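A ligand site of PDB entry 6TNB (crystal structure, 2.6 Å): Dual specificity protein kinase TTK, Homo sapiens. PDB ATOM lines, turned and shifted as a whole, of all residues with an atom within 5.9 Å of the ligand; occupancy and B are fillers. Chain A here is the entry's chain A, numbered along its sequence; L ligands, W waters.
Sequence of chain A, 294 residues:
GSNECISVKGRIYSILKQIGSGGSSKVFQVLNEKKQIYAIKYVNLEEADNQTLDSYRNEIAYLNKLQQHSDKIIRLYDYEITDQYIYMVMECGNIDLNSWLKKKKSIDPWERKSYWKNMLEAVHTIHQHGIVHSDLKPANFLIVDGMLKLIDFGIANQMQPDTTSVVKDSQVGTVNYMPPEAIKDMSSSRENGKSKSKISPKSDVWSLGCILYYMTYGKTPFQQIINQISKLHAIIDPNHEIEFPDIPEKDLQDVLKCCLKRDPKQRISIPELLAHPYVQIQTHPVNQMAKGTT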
ATOM      1  N   LYS A  17       8.985 -27.270  24.382  1.00  0.00           N
ATOM      2  CA  LYS A  17       7.656 -26.598  24.293  1.00  0.00           C
ATOM      3  C   LYS A  17       7.752 -25.303  23.502  1.00  0.00           C
ATOM      4  O   LYS A  17       8.847 -24.714  23.409  1.00  0.00           O
ATOM      5  CB  LYS A  17       7.094 -26.303  25.690  1.00  0.00           C
ATOM      6  CG  LYS A  17       8.149 -25.826  26.684  1.00  0.00           C
ATOM      7  CD  LYS A  17       7.613 -24.907  27.759  1.00  0.00           C
ATOM      8  CE  LYS A  17       8.684 -24.485  28.740  1.00  0.00           C
ATOM      9  NZ  LYS A  17       8.275 -23.295  29.518  1.00  0.00           N
ATOM     10  N   ILE A  19       7.026 -21.372  23.403  1.00  0.00           N
ATOM     11  CA  ILE A  19       7.343 -20.236  24.315  1.00  0.00           C
ATOM     12  C   ILE A  19       6.828 -18.931  23.714  1.00  0.00           C
ATOM     13  O   ILE A  19       6.557 -17.970  24.455  1.00  0.00           O
ATOM     14  CB  ILE A  19       8.867 -20.104  24.494  1.00  0.00           C
ATOM     15  CG1 ILE A  19       9.502 -21.371  25.082  1.00  0.00           C
ATOM     16  CG2 ILE A  19       9.147 -18.872  25.311  1.00  0.00           C
ATOM     17  CD1 ILE A  19      11.008 -21.317  25.108  1.00  0.00           C
ATOM     18  N   VAL A  27       8.489 -19.484  18.766  1.00  0.00           N
ATOM     19  CA  VAL A  27       9.763 -19.708  19.513  1.00  0.00           C
ATOM     20  C   VAL A  27       9.579 -21.017  20.281  1.00  0.00           C
ATOM     21  O   VAL A  27       8.524 -21.209  20.886  1.00  0.00           O
ATOM     22  CB  VAL A  27      10.135 -18.561  20.481  1.00  0.00           C
ATOM     23  CG1 VAL A  27      11.589 -18.648  20.900  1.00  0.00           C
ATOM     24  CG2 VAL A  27       9.815 -17.172  19.948  1.00  0.00           C
ATOM     25  N   GLN A  29      11.471 -23.770  23.078  1.00  0.00           N
ATOM     26  CA  GLN A  29      12.490 -24.380  23.977  1.00  0.00           C
ATOM     27  C   GLN A  29      12.830 -25.759  23.410  1.00  0.00           C
ATOM     28  O   GLN A  29      11.944 -26.389  22.846  1.00  0.00           O
ATOM     29  CB  GLN A  29      11.966 -24.478  25.407  1.00  0.00           C
ATOM     30  CG  GLN A  29      13.007 -24.032  26.422  1.00  0.00           C
ATOM     31  CD  GLN A  29      12.986 -24.896  27.648  1.00  0.00           C
ATOM     32  OE1 GLN A  29      13.994 -25.547  27.952  1.00  0.00           O
ATOM     33  NE2 GLN A  29      11.846 -24.913  28.322  1.00  0.00           N
ATOM     34  N   ALA A  39      16.676 -21.856  22.579  1.00  0.00           N
ATOM     35  CA  ALA A  39      15.435 -21.308  21.996  1.00  0.00           C
ATOM     36  C   ALA A  39      15.659 -21.301  20.490  1.00  0.00           C
ATOM     37  O   ALA A  39      16.765 -20.948  20.068  1.00  0.00           O
ATOM     38  CB  ALA A  39      15.104 -19.951  22.535  1.00  0.00           C
ATOM     39  N   LYS A  41      13.724 -19.860  16.979  1.00  0.00           N
ATOM     40  CA  LYS A  41      12.625 -19.061  16.408  1.00  0.00           C
ATOM     41  C   LYS A  41      12.396 -19.551  14.979  1.00  0.00           C
ATOM     42  O   LYS A  41      13.377 -19.615  14.247  1.00  0.00           O
ATOM     43  CB  LYS A  41      12.939 -17.571  16.394  1.00  0.00           C
ATOM     44  CG  LYS A  41      11.677 -16.780  16.105  1.00  0.00           C
ATOM     45  CD  LYS A  41      11.865 -15.352  15.755  1.00  0.00           C
ATOM     46  CE  LYS A  41      10.560 -14.842  15.166  1.00  0.00           C
ATOM     47  NZ  LYS A  41      10.117 -13.559  15.768  1.00  0.00           N
ATOM     48  N   VAL A  43      10.236 -18.714  11.543  1.00  0.00           N
ATOM     49  CA  VAL A  43       9.410 -17.762  10.733  1.00  0.00           C
ATOM     50  C   VAL A  43       9.035 -18.442   9.402  1.00  0.00           C
ATOM     51  O   VAL A  43       9.908 -19.084   8.787  1.00  0.00           O
ATOM     52  CB  VAL A  43      10.141 -16.441  10.523  1.00  0.00           C
ATOM     53  CG1 VAL A  43       9.172 -15.361  10.060  1.00  0.00           C
ATOM     54  CG2 VAL A  43      10.874 -16.019  11.793  1.00  0.00           C
ATOM     55  N   TYR A  56      13.539  -8.800   7.513  1.00  0.00           N
ATOM     56  CA  TYR A  56      14.052 -10.029   8.170  1.00  0.00           C
ATOM     57  C   TYR A  56      15.553 -10.139   7.907  1.00  0.00           C
ATOM     58  O   TYR A  56      16.333 -10.259   8.874  1.00  0.00           O
ATOM     59  CB  TYR A  56      13.313 -11.257   7.659  1.00  0.00           C
ATOM     60  CG  TYR A  56      11.843 -11.321   8.012  1.00  0.00           C
ATOM     61  CD1 TYR A  56      11.278 -10.507   8.985  1.00  0.00           C
ATOM     62  CD2 TYR A  56      11.023 -12.248   7.375  1.00  0.00           C
ATOM     63  CE1 TYR A  56       9.925 -10.599   9.300  1.00  0.00           C
ATOM     64  CE2 TYR A  56       9.677 -12.349   7.681  1.00  0.00           C
ATOM     65  CZ  TYR A  56       9.128 -11.524   8.644  1.00  0.00           C
ATOM     66  OH  TYR A  56       7.819 -11.663   8.956  1.00  0.00           O
ATOM     67  N   ARG A  57      15.942 -10.064   6.638  1.00  0.00           N
ATOM     68  CA  ARG A  57      17.346 -10.206   6.201  1.00  0.00           C
ATOM     69  C   ARG A  57      18.231  -9.191   6.958  1.00  0.00           C
ATOM     70  O   ARG A  57      19.373  -9.553   7.364  1.00  0.00           O
ATOM     71  CB  ARG A  57      17.407 -10.007   4.677  1.00  0.00           C
ATOM     72  CG  ARG A  57      16.818 -11.138   3.855  1.00  0.00           C
ATOM     73  CD  ARG A  57      16.542 -10.713   2.436  1.00  0.00           C
ATOM     74  NE  ARG A  57      16.364 -11.816   1.496  1.00  0.00           N
ATOM     75  CZ  ARG A  57      15.457 -11.833   0.524  1.00  0.00           C
ATOM     76  NH1 ARG A  57      14.633 -10.821   0.351  1.00  0.00           N
ATOM     77  NH2 ARG A  57      15.375 -12.877  -0.279  1.00  0.00           N
ATOM     78  N   GLU A  59      17.404  -7.288   9.962  1.00  0.00           N
ATOM     79  CA  GLU A  59      17.413  -7.600  11.403  1.00  0.00           C
ATOM     80  C   GLU A  59      18.433  -8.718  11.610  1.00  0.00           C
ATOM     81  O   GLU A  59      19.301  -8.558  12.442  1.00  0.00           O
ATOM     82  CB  GLU A  59      16.030  -8.018  11.882  1.00  0.00           C
ATOM     83  CG  GLU A  59      16.036  -8.424  13.335  1.00  0.00           C
ATOM     84  CD  GLU A  59      15.570  -7.377  14.322  1.00  0.00           C
ATOM     85  OE1 GLU A  59      14.722  -6.537  13.950  1.00  0.00           O
ATOM     86  OE2 GLU A  59      16.045  -7.414  15.455  1.00  0.00           O
ATOM     87  N   ILE A  60      18.357  -9.802  10.849  1.00  0.00           N
ATOM     88  CA  ILE A  60      19.237 -10.994  11.060  1.00  0.00           C
ATOM     89  C   ILE A  60      20.681 -10.560  10.822  1.00  0.00           C
ATOM     90  O   ILE A  60      21.506 -10.777  11.693  1.00  0.00           O
ATOM     91  CB  ILE A  60      18.804 -12.187  10.193  1.00  0.00           C
ATOM     92  CG1 ILE A  60      17.583 -12.879  10.801  1.00  0.00           C
ATOM     93  CG2 ILE A  60      19.949 -13.173   9.988  1.00  0.00           C
ATOM     94  CD1 ILE A  60      16.674 -13.578   9.824  1.00  0.00           C
ATOM     95  N   LEU A  63      21.850  -8.586  13.795  1.00  0.00           N
ATOM     96  CA  LEU A  63      21.864  -9.406  15.034  1.00  0.00           C
ATOM     97  C   LEU A  63      23.063 -10.369  14.939  1.00  0.00           C
ATOM     98  O   LEU A  63      23.879 -10.460  15.879  1.00  0.00           O
ATOM     99  CB  LEU A  63      20.494 -10.111  15.126  1.00  0.00           C
ATOM    100  CG  LEU A  63      20.100 -10.814  16.432  1.00  0.00           C
ATOM    101  CD1 LEU A  63      20.135 -12.320  16.256  1.00  0.00           C
ATOM    102  CD2 LEU A  63      20.952 -10.389  17.614  1.00  0.00           C
ATOM    103  N   ILE A  74      21.108 -10.675  22.641  1.00  0.00           N
ATOM    104  CA  ILE A  74      20.760 -12.125  22.671  1.00  0.00           C
ATOM    105  C   ILE A  74      21.753 -12.887  21.784  1.00  0.00           C
ATOM    106  O   ILE A  74      21.854 -12.557  20.625  1.00  0.00           O
ATOM    107  CB  ILE A  74      19.305 -12.343  22.219  1.00  0.00           C
ATOM    108  CG1 ILE A  74      18.830 -13.760  22.579  1.00  0.00           C
ATOM    109  CG2 ILE A  74      19.121 -12.012  20.722  1.00  0.00           C
ATOM    110  CD1 ILE A  74      18.598 -13.956  24.066  1.00  0.00           C
ATOM    111  N   ILE A  86      12.638 -19.369   7.952  1.00  0.00           N
ATOM    112  CA  ILE A  86      13.825 -19.053   8.795  1.00  0.00           C
ATOM    113  C   ILE A  86      13.765 -19.833  10.121  1.00  0.00           C
ATOM    114  O   ILE A  86      12.704 -19.781  10.780  1.00  0.00           O
ATOM    115  CB  ILE A  86      13.910 -17.548   9.073  1.00  0.00           C
ATOM    116  CG1 ILE A  86      14.091 -16.736   7.783  1.00  0.00           C
ATOM    117  CG2 ILE A  86      15.028 -17.279  10.069  1.00  0.00           C
ATOM    118  CD1 ILE A  86      13.942 -15.259   7.990  1.00  0.00           C
ATOM    119  N   MET A  88      16.274 -19.581  13.603  1.00  0.00           N
ATOM    120  CA  MET A  88      17.359 -18.927  14.381  1.00  0.00           C
ATOM    121  C   MET A  88      17.569 -19.683  15.698  1.00  0.00           C
ATOM    122  O   MET A  88      16.651 -19.668  16.537  1.00  0.00           O
ATOM    123  CB  MET A  88      16.965 -17.482  14.698  1.00  0.00           C
ATOM    124  CG  MET A  88      16.976 -16.555  13.503  1.00  0.00           C
ATOM    125  SD  MET A  88      15.911 -15.134  13.742  1.00  0.00           S
ATOM    126  CE  MET A  88      16.852 -14.210  14.947  1.00  0.00           C
ATOM    127  N   MET A  90      19.440 -19.917  19.242  1.00  0.00           N
ATOM    128  CA  MET A  90      19.781 -18.823  20.166  1.00  0.00           C
ATOM    129  C   MET A  90      19.903 -19.374  21.596  1.00  0.00           C
ATOM    130  O   MET A  90      19.187 -20.342  21.963  1.00  0.00           O
ATOM    131  CB  MET A  90      18.683 -17.751  20.126  1.00  0.00           C
ATOM    132  CG  MET A  90      18.514 -17.064  18.772  1.00  0.00           C
ATOM    133  SD  MET A  90      17.386 -15.620  18.787  1.00  0.00           S
ATOM    134  CE  MET A  90      15.804 -16.427  18.558  1.00  0.00           C
ATOM    135  N   GLU A  91      20.747 -18.779  22.427  1.00  0.00           N
ATOM    136  CA  GLU A  91      20.702 -19.002  23.887  1.00  0.00           C
ATOM    137  C   GLU A  91      19.241 -18.844  24.348  1.00  0.00           C
ATOM    138  O   GLU A  91      18.493 -18.015  23.738  1.00  0.00           O
ATOM    139  CB  GLU A  91      21.630 -18.055  24.629  1.00  0.00           C
ATOM    140  CG  GLU A  91      21.046 -16.682  24.860  1.00  0.00           C
ATOM    141  CD  GLU A  91      22.055 -15.675  25.380  1.00  0.00           C
ATOM    142  OE1 GLU A  91      21.958 -14.509  24.977  1.00  0.00           O
ATOM    143  OE2 GLU A  91      22.966 -16.064  26.169  1.00  0.00           O
ATOM    144  N   CYS A  92      18.847 -19.613  25.359  1.00  0.00           N
ATOM    145  CA  CYS A  92      17.445 -19.671  25.826  1.00  0.00           C
ATOM    146  C   CYS A  92      17.269 -18.823  27.084  1.00  0.00           C
ATOM    147  O   CYS A  92      18.110 -18.925  27.986  1.00  0.00           O
ATOM    148  CB  CYS A  92      16.955 -21.100  26.080  1.00  0.00           C
ATOM    149  SG  CYS A  92      15.165 -21.142  26.378  1.00  0.00           S
ATOM    150  N   GLY A  93      16.178 -18.083  27.150  1.00  0.00           N
ATOM    151  CA  GLY A  93      15.863 -17.202  28.285  1.00  0.00           C
ATOM    152  C   GLY A  93      15.257 -17.965  29.447  1.00  0.00           C
ATOM    153  O   GLY A  93      15.052 -19.183  29.346  1.00  0.00           O
ATOM    154  N   ASN A  94      15.019 -17.236  30.540  1.00  0.00           N
ATOM    155  CA  ASN A  94      14.153 -17.645  31.670  1.00  0.00           C
ATOM    156  C   ASN A  94      12.760 -17.089  31.380  1.00  0.00           C
ATOM    157  O   ASN A  94      11.809 -17.867  31.403  1.00  0.00           O
ATOM    158  CB  ASN A  94      14.712 -17.158  33.013  1.00  0.00           C
ATOM    159  CG  ASN A  94      16.211 -17.398  33.155  1.00  0.00           C
ATOM    160  OD1 ASN A  94      16.861 -17.950  32.267  1.00  0.00           O
ATOM    161  ND2 ASN A  94      16.777 -16.949  34.270  1.00  0.00           N
ATOM    162  N   ILE A  95      12.684 -15.803  31.038  1.00  0.00           N
ATOM    163  CA  ILE A  95      11.393 -15.049  30.907  1.00  0.00           C
ATOM    164  C   ILE A  95      11.641 -13.659  30.286  1.00  0.00           C
ATOM    165  O   ILE A  95      12.728 -13.088  30.474  1.00  0.00           O
ATOM    166  CB  ILE A  95      10.723 -14.962  32.282  1.00  0.00           C
ATOM    167  CG1 ILE A  95       9.489 -14.046  32.260  1.00  0.00           C
ATOM    168  CG2 ILE A  95      11.752 -14.543  33.326  1.00  0.00           C
ATOM    169  CD1 ILE A  95       8.792 -13.874  33.589  1.00  0.00           C
ATOM    170  N   ASP A  96      10.638 -13.116  29.590  1.00  0.00           N
ATOM    171  CA  ASP A  96      10.721 -11.763  28.974  1.00  0.00           C
ATOM    172  C   ASP A  96      10.574 -10.778  30.130  1.00  0.00           C
ATOM    173  O   ASP A  96      10.555 -11.228  31.263  1.00  0.00           O
ATOM    174  CB  ASP A  96       9.748 -11.613  27.800  1.00  0.00           C
ATOM    175  CG  ASP A  96       8.414 -10.938  28.062  1.00  0.00           C
ATOM    176  OD1 ASP A  96       8.402  -9.744  28.423  1.00  0.00           O
ATOM    177  OD2 ASP A  96       7.387 -11.609  27.846  1.00  0.00           O
ATOM    178  N   SER A  99       6.301  -9.866  31.029  1.00  0.00           N
ATOM    179  CA  SER A  99       6.034 -10.970  31.992  1.00  0.00           C
ATOM    180  C   SER A  99       6.488 -10.588  33.412  1.00  0.00           C
ATOM    181  O   SER A  99       5.631 -10.442  34.318  1.00  0.00           O
ATOM    182  CB  SER A  99       6.707 -12.272  31.579  1.00  0.00           C
ATOM    183  OG  SER A  99       6.248 -12.756  30.329  1.00  0.00           O
ATOM    184  N   LEU A 142      14.852  -9.620  27.506  1.00  0.00           N
ATOM    185  CA  LEU A 142      14.765 -11.017  27.936  1.00  0.00           C
ATOM    186  C   LEU A 142      15.820 -11.236  29.024  1.00  0.00           C
ATOM    187  O   LEU A 142      16.970 -10.869  28.790  1.00  0.00           O
ATOM    188  CB  LEU A 142      15.061 -11.901  26.726  1.00  0.00           C
ATOM    189  CG  LEU A 142      14.878 -13.391  26.966  1.00  0.00           C
ATOM    190  CD1 LEU A 142      13.414 -13.759  26.803  1.00  0.00           C
ATOM    191  CD2 LEU A 142      15.771 -14.235  26.060  1.00  0.00           C
ATOM    192  N   ILE A 151      16.820  -8.517  22.228  1.00  0.00           N
ATOM    193  CA  ILE A 151      16.617  -9.701  21.361  1.00  0.00           C
ATOM    194  C   ILE A 151      16.270  -9.240  19.948  1.00  0.00           C
ATOM    195  O   ILE A 151      16.295 -10.106  19.043  1.00  0.00           O
ATOM    196  CB  ILE A 151      15.497 -10.586  21.940  1.00  0.00           C
ATOM    197  CG1 ILE A 151      14.260  -9.761  22.304  1.00  0.00           C
ATOM    198  CG2 ILE A 151      16.010 -11.372  23.133  1.00  0.00           C
ATOM    199  CD1 ILE A 151      12.993 -10.537  22.304  1.00  0.00           C
ATOM    200  N   ASP A 152      15.952  -7.968  19.765  1.00  0.00           N
ATOM    201  CA  ASP A 152      15.621  -7.419  18.419  1.00  0.00           C
ATOM    202  C   ASP A 152      15.906  -5.907  18.321  1.00  0.00           C
ATOM    203  O   ASP A 152      16.129  -5.237  19.358  1.00  0.00           O
ATOM    204  CB  ASP A 152      14.163  -7.729  18.096  1.00  0.00           C
ATOM    205  CG  ASP A 152      13.246  -6.875  18.923  1.00  0.00           C
ATOM    206  OD1 ASP A 152      13.714  -6.388  19.969  1.00  0.00           O
ATOM    207  OD2 ASP A 152      12.107  -6.661  18.509  1.00  0.00           O
ATOM    208  N   ALA A 156      12.957  -5.676  11.527  1.00  0.00           N
ATOM    209  CA  ALA A 156      11.930  -6.666  11.098  1.00  0.00           C
ATOM    210  C   ALA A 156      10.537  -6.201  11.567  1.00  0.00           C
ATOM    211  O   ALA A 156      10.474  -5.291  12.416  1.00  0.00           O
ATOM    212  CB  ALA A 156      12.283  -7.997  11.684  1.00  0.00           C
ATOM    213  N   ASN A 157       9.475  -6.805  11.037  1.00  0.00           N
ATOM    214  CA  ASN A 157       8.087  -6.290  11.234  1.00  0.00           C
ATOM    215  C   ASN A 157       7.141  -7.471  11.505  1.00  0.00           C
ATOM    216  O   ASN A 157       6.295  -7.325  12.418  1.00  0.00           O
ATOM    217  CB  ASN A 157       7.676  -5.378  10.071  1.00  0.00           C
ATOM    218  CG  ASN A 157       8.035  -5.916   8.689  1.00  0.00           C
ATOM    219  OD1 ASN A 157       8.472  -5.173   7.805  1.00  0.00           O
ATOM    220  ND2 ASN A 157       7.855  -7.201   8.485  1.00  0.00           N
HETATM  221  C1  LIG L   1      14.613 -16.796  23.918  1.00  0.00           C
HETATM  222  C2  LIG L   1      15.462 -15.788  21.953  1.00  0.00           C
HETATM  223  C3  LIG L   1      14.248 -15.091  21.731  1.00  0.00           C
HETATM  224  C4  LIG L   1      13.192 -15.284  22.606  1.00  0.00           C
HETATM  225  C5  LIG L   1      11.576 -17.678  27.187  1.00  0.00           C
HETATM  226  C6  LIG L   1       9.597 -16.375  27.620  1.00  0.00           C
HETATM  227  C7  LIG L   1      10.815 -16.519  26.989  1.00  0.00           C
HETATM  228  C8  LIG L   1       9.092 -17.395  28.444  1.00  0.00           C
HETATM  229  C9  LIG L   1      11.080 -18.706  28.025  1.00  0.00           C
HETATM  230  F1  LIG L   1      13.279 -13.152  10.602  1.00  0.00           F
HETATM  231  C10 LIG L   1      13.058 -12.463  11.744  1.00  0.00           C
HETATM  232  C11 LIG L   1      11.825 -11.828  11.980  1.00  0.00           C
HETATM  233  C12 LIG L   1      11.647 -11.133  13.199  1.00  0.00           C
HETATM  234  C13 LIG L   1      14.085 -12.429  12.690  1.00  0.00           C
HETATM  235  C14 LIG L   1      13.917 -11.732  13.881  1.00  0.00           C
HETATM  236  C15 LIG L   1      12.708 -11.097  14.133  1.00  0.00           C
HETATM  237  C16 LIG L   1      12.552 -10.351  15.447  1.00  0.00           C
HETATM  238  C17 LIG L   1      11.199  -9.609  15.331  1.00  0.00           C
HETATM  239  C18 LIG L   1      12.520 -11.321  16.660  1.00  0.00           C
HETATM  240  O1  LIG L   1      11.424 -11.654  17.080  1.00  0.00           O
HETATM  241  N1  LIG L   1      13.683 -11.752  17.210  1.00  0.00           N
HETATM  242  C19 LIG L   1      13.804 -12.583  18.313  1.00  0.00           C
HETATM  243  C20 LIG L   1      15.094 -12.968  18.750  1.00  0.00           C
HETATM  244  C21 LIG L   1      15.234 -13.787  19.864  1.00  0.00           C
HETATM  245  C22 LIG L   1      14.110 -14.244  20.602  1.00  0.00           C
HETATM  246  C23 LIG L   1      12.838 -13.851  20.190  1.00  0.00           C
HETATM  247  C24 LIG L   1      12.693 -13.019  19.071  1.00  0.00           C
HETATM  248  N2  LIG L   1      13.345 -16.141  23.711  1.00  0.00           N
HETATM  249  C25 LIG L   1      15.660 -16.602  23.057  1.00  0.00           C
HETATM  250  N3  LIG L   1      14.517 -17.523  25.006  1.00  0.00           N
HETATM  251  C26 LIG L   1      13.244 -17.302  25.441  1.00  0.00           C
HETATM  252  N4  LIG L   1      12.557 -16.452  24.613  1.00  0.00           N
HETATM  253  N5  LIG L   1      12.780 -17.898  26.588  1.00  0.00           N
HETATM  254  O2  LIG L   1      11.872 -19.840  28.166  1.00  0.00           O
HETATM  255  C27 LIG L   1      11.398 -20.799  29.125  1.00  0.00           C
HETATM  256  C28 LIG L   1       9.825 -18.568  28.660  1.00  0.00           C
HETATM  257  S1  LIG L   1       7.508 -17.201  29.244  1.00  0.00           S
HETATM  258  C29 LIG L   1       6.242 -18.156  28.409  1.00  0.00           C
HETATM  259  O3  LIG L   1       7.088 -15.728  29.333  1.00  0.00           O
HETATM  260  O4  LIG L   1       7.765 -17.762  30.597  1.00  0.00           O
HETATM  261  O   HOH W   1      16.171 -10.120  16.542  1.00  0.00           O
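An oxygen (O1) of the ligand is in hydrogen-bond range of the side-chain amino group (NZ) of Lys 41, at 2.7 Å.
N3 of the ligand sits at hydrogen-bond distance from N of Gly 93 (2.8 Å).
OG of Ser 99 lies within hydrogen-bond range of O3 of the ligand (3.2 Å).
N of Lys 41 is in hydrogen-bond range of O of Met 88 (3.0 Å).
The backbone NH (N) of Met 90 sits at hydrogen-bond distance from the backbone carbonyl oxygen (O) of Ala 39 (3.0 Å).
OD2 of Asp 96 lies within hydrogen-bond range of OG of Ser 99, at 3.0 Å.
O of Val 27 sits at hydrogen-bond distance from N of Ile 19, at 2.9 Å.
O of Ile 86 sits at hydrogen-bond distance from N of Val 43.
The backbone NH (N) of Ala 156 lies within hydrogen-bond range of the side-chain carboxylate (OE1) of Glu 59 (3.1 Å).
Ile 19 touches the ligand (CG2 to C5, 3.3 Å).
Ala 39 touches the ligand.
CG2 of Val 43 touches F1 of the ligand, 3.9 Å away.
CD1 of Tyr 56 touches C11 of the ligand (3.3 Å).
Glu 59 touches the ligand.
Ile 60 touches the ligand (CD1 to F1, 3.5 Å).
Ile 74 touches the ligand (CG1 to C2, 3.98 Å).
Ile 86 touches the ligand (CD1 to F1, 3.4 Å).
SD of Met 88 touches C13 of the ligand (3.4 Å).
CE of Met 90 touches C21 of the ligand (3.0 Å).
Glu 91 touches the ligand.
Cys 92 touches the ligand (C to N3, 3.7 Å).
O of Asn 94 touches C28 of the ligand (3.5 Å).
Ile 95 touches the ligand.
N of Asp 96 touches C6 of the ligand (3.9 Å).
Leu 142 touches the ligand.
O of Ile 151 touches C20 of the ligand (3.1 Å).
CB of Ala 156 touches C12 of the ligand, at 3.5 Å.
Within 4 Å of the ligand: Ile 19, Ala 39, Lys 41, Val 43, Tyr 56, Glu 59, Ile 60, Ile 74, Ile 86, Met 88, Met 90, Glu 91, Cys 92, Gly 93, Asn 94, Ile 95, Asp 96, Ser 99, Leu 142, Ile 151 and Ala 156.
Water W1 lies within hydrogen-bond range of the backbone carbonyl oxygen (O) of Ile 151 (2.5 Å), the side-chain carboxylate (OE2) of Glu 59 (2.9 Å) and a nitrogen (N1) of the ligand (3.0 Å).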
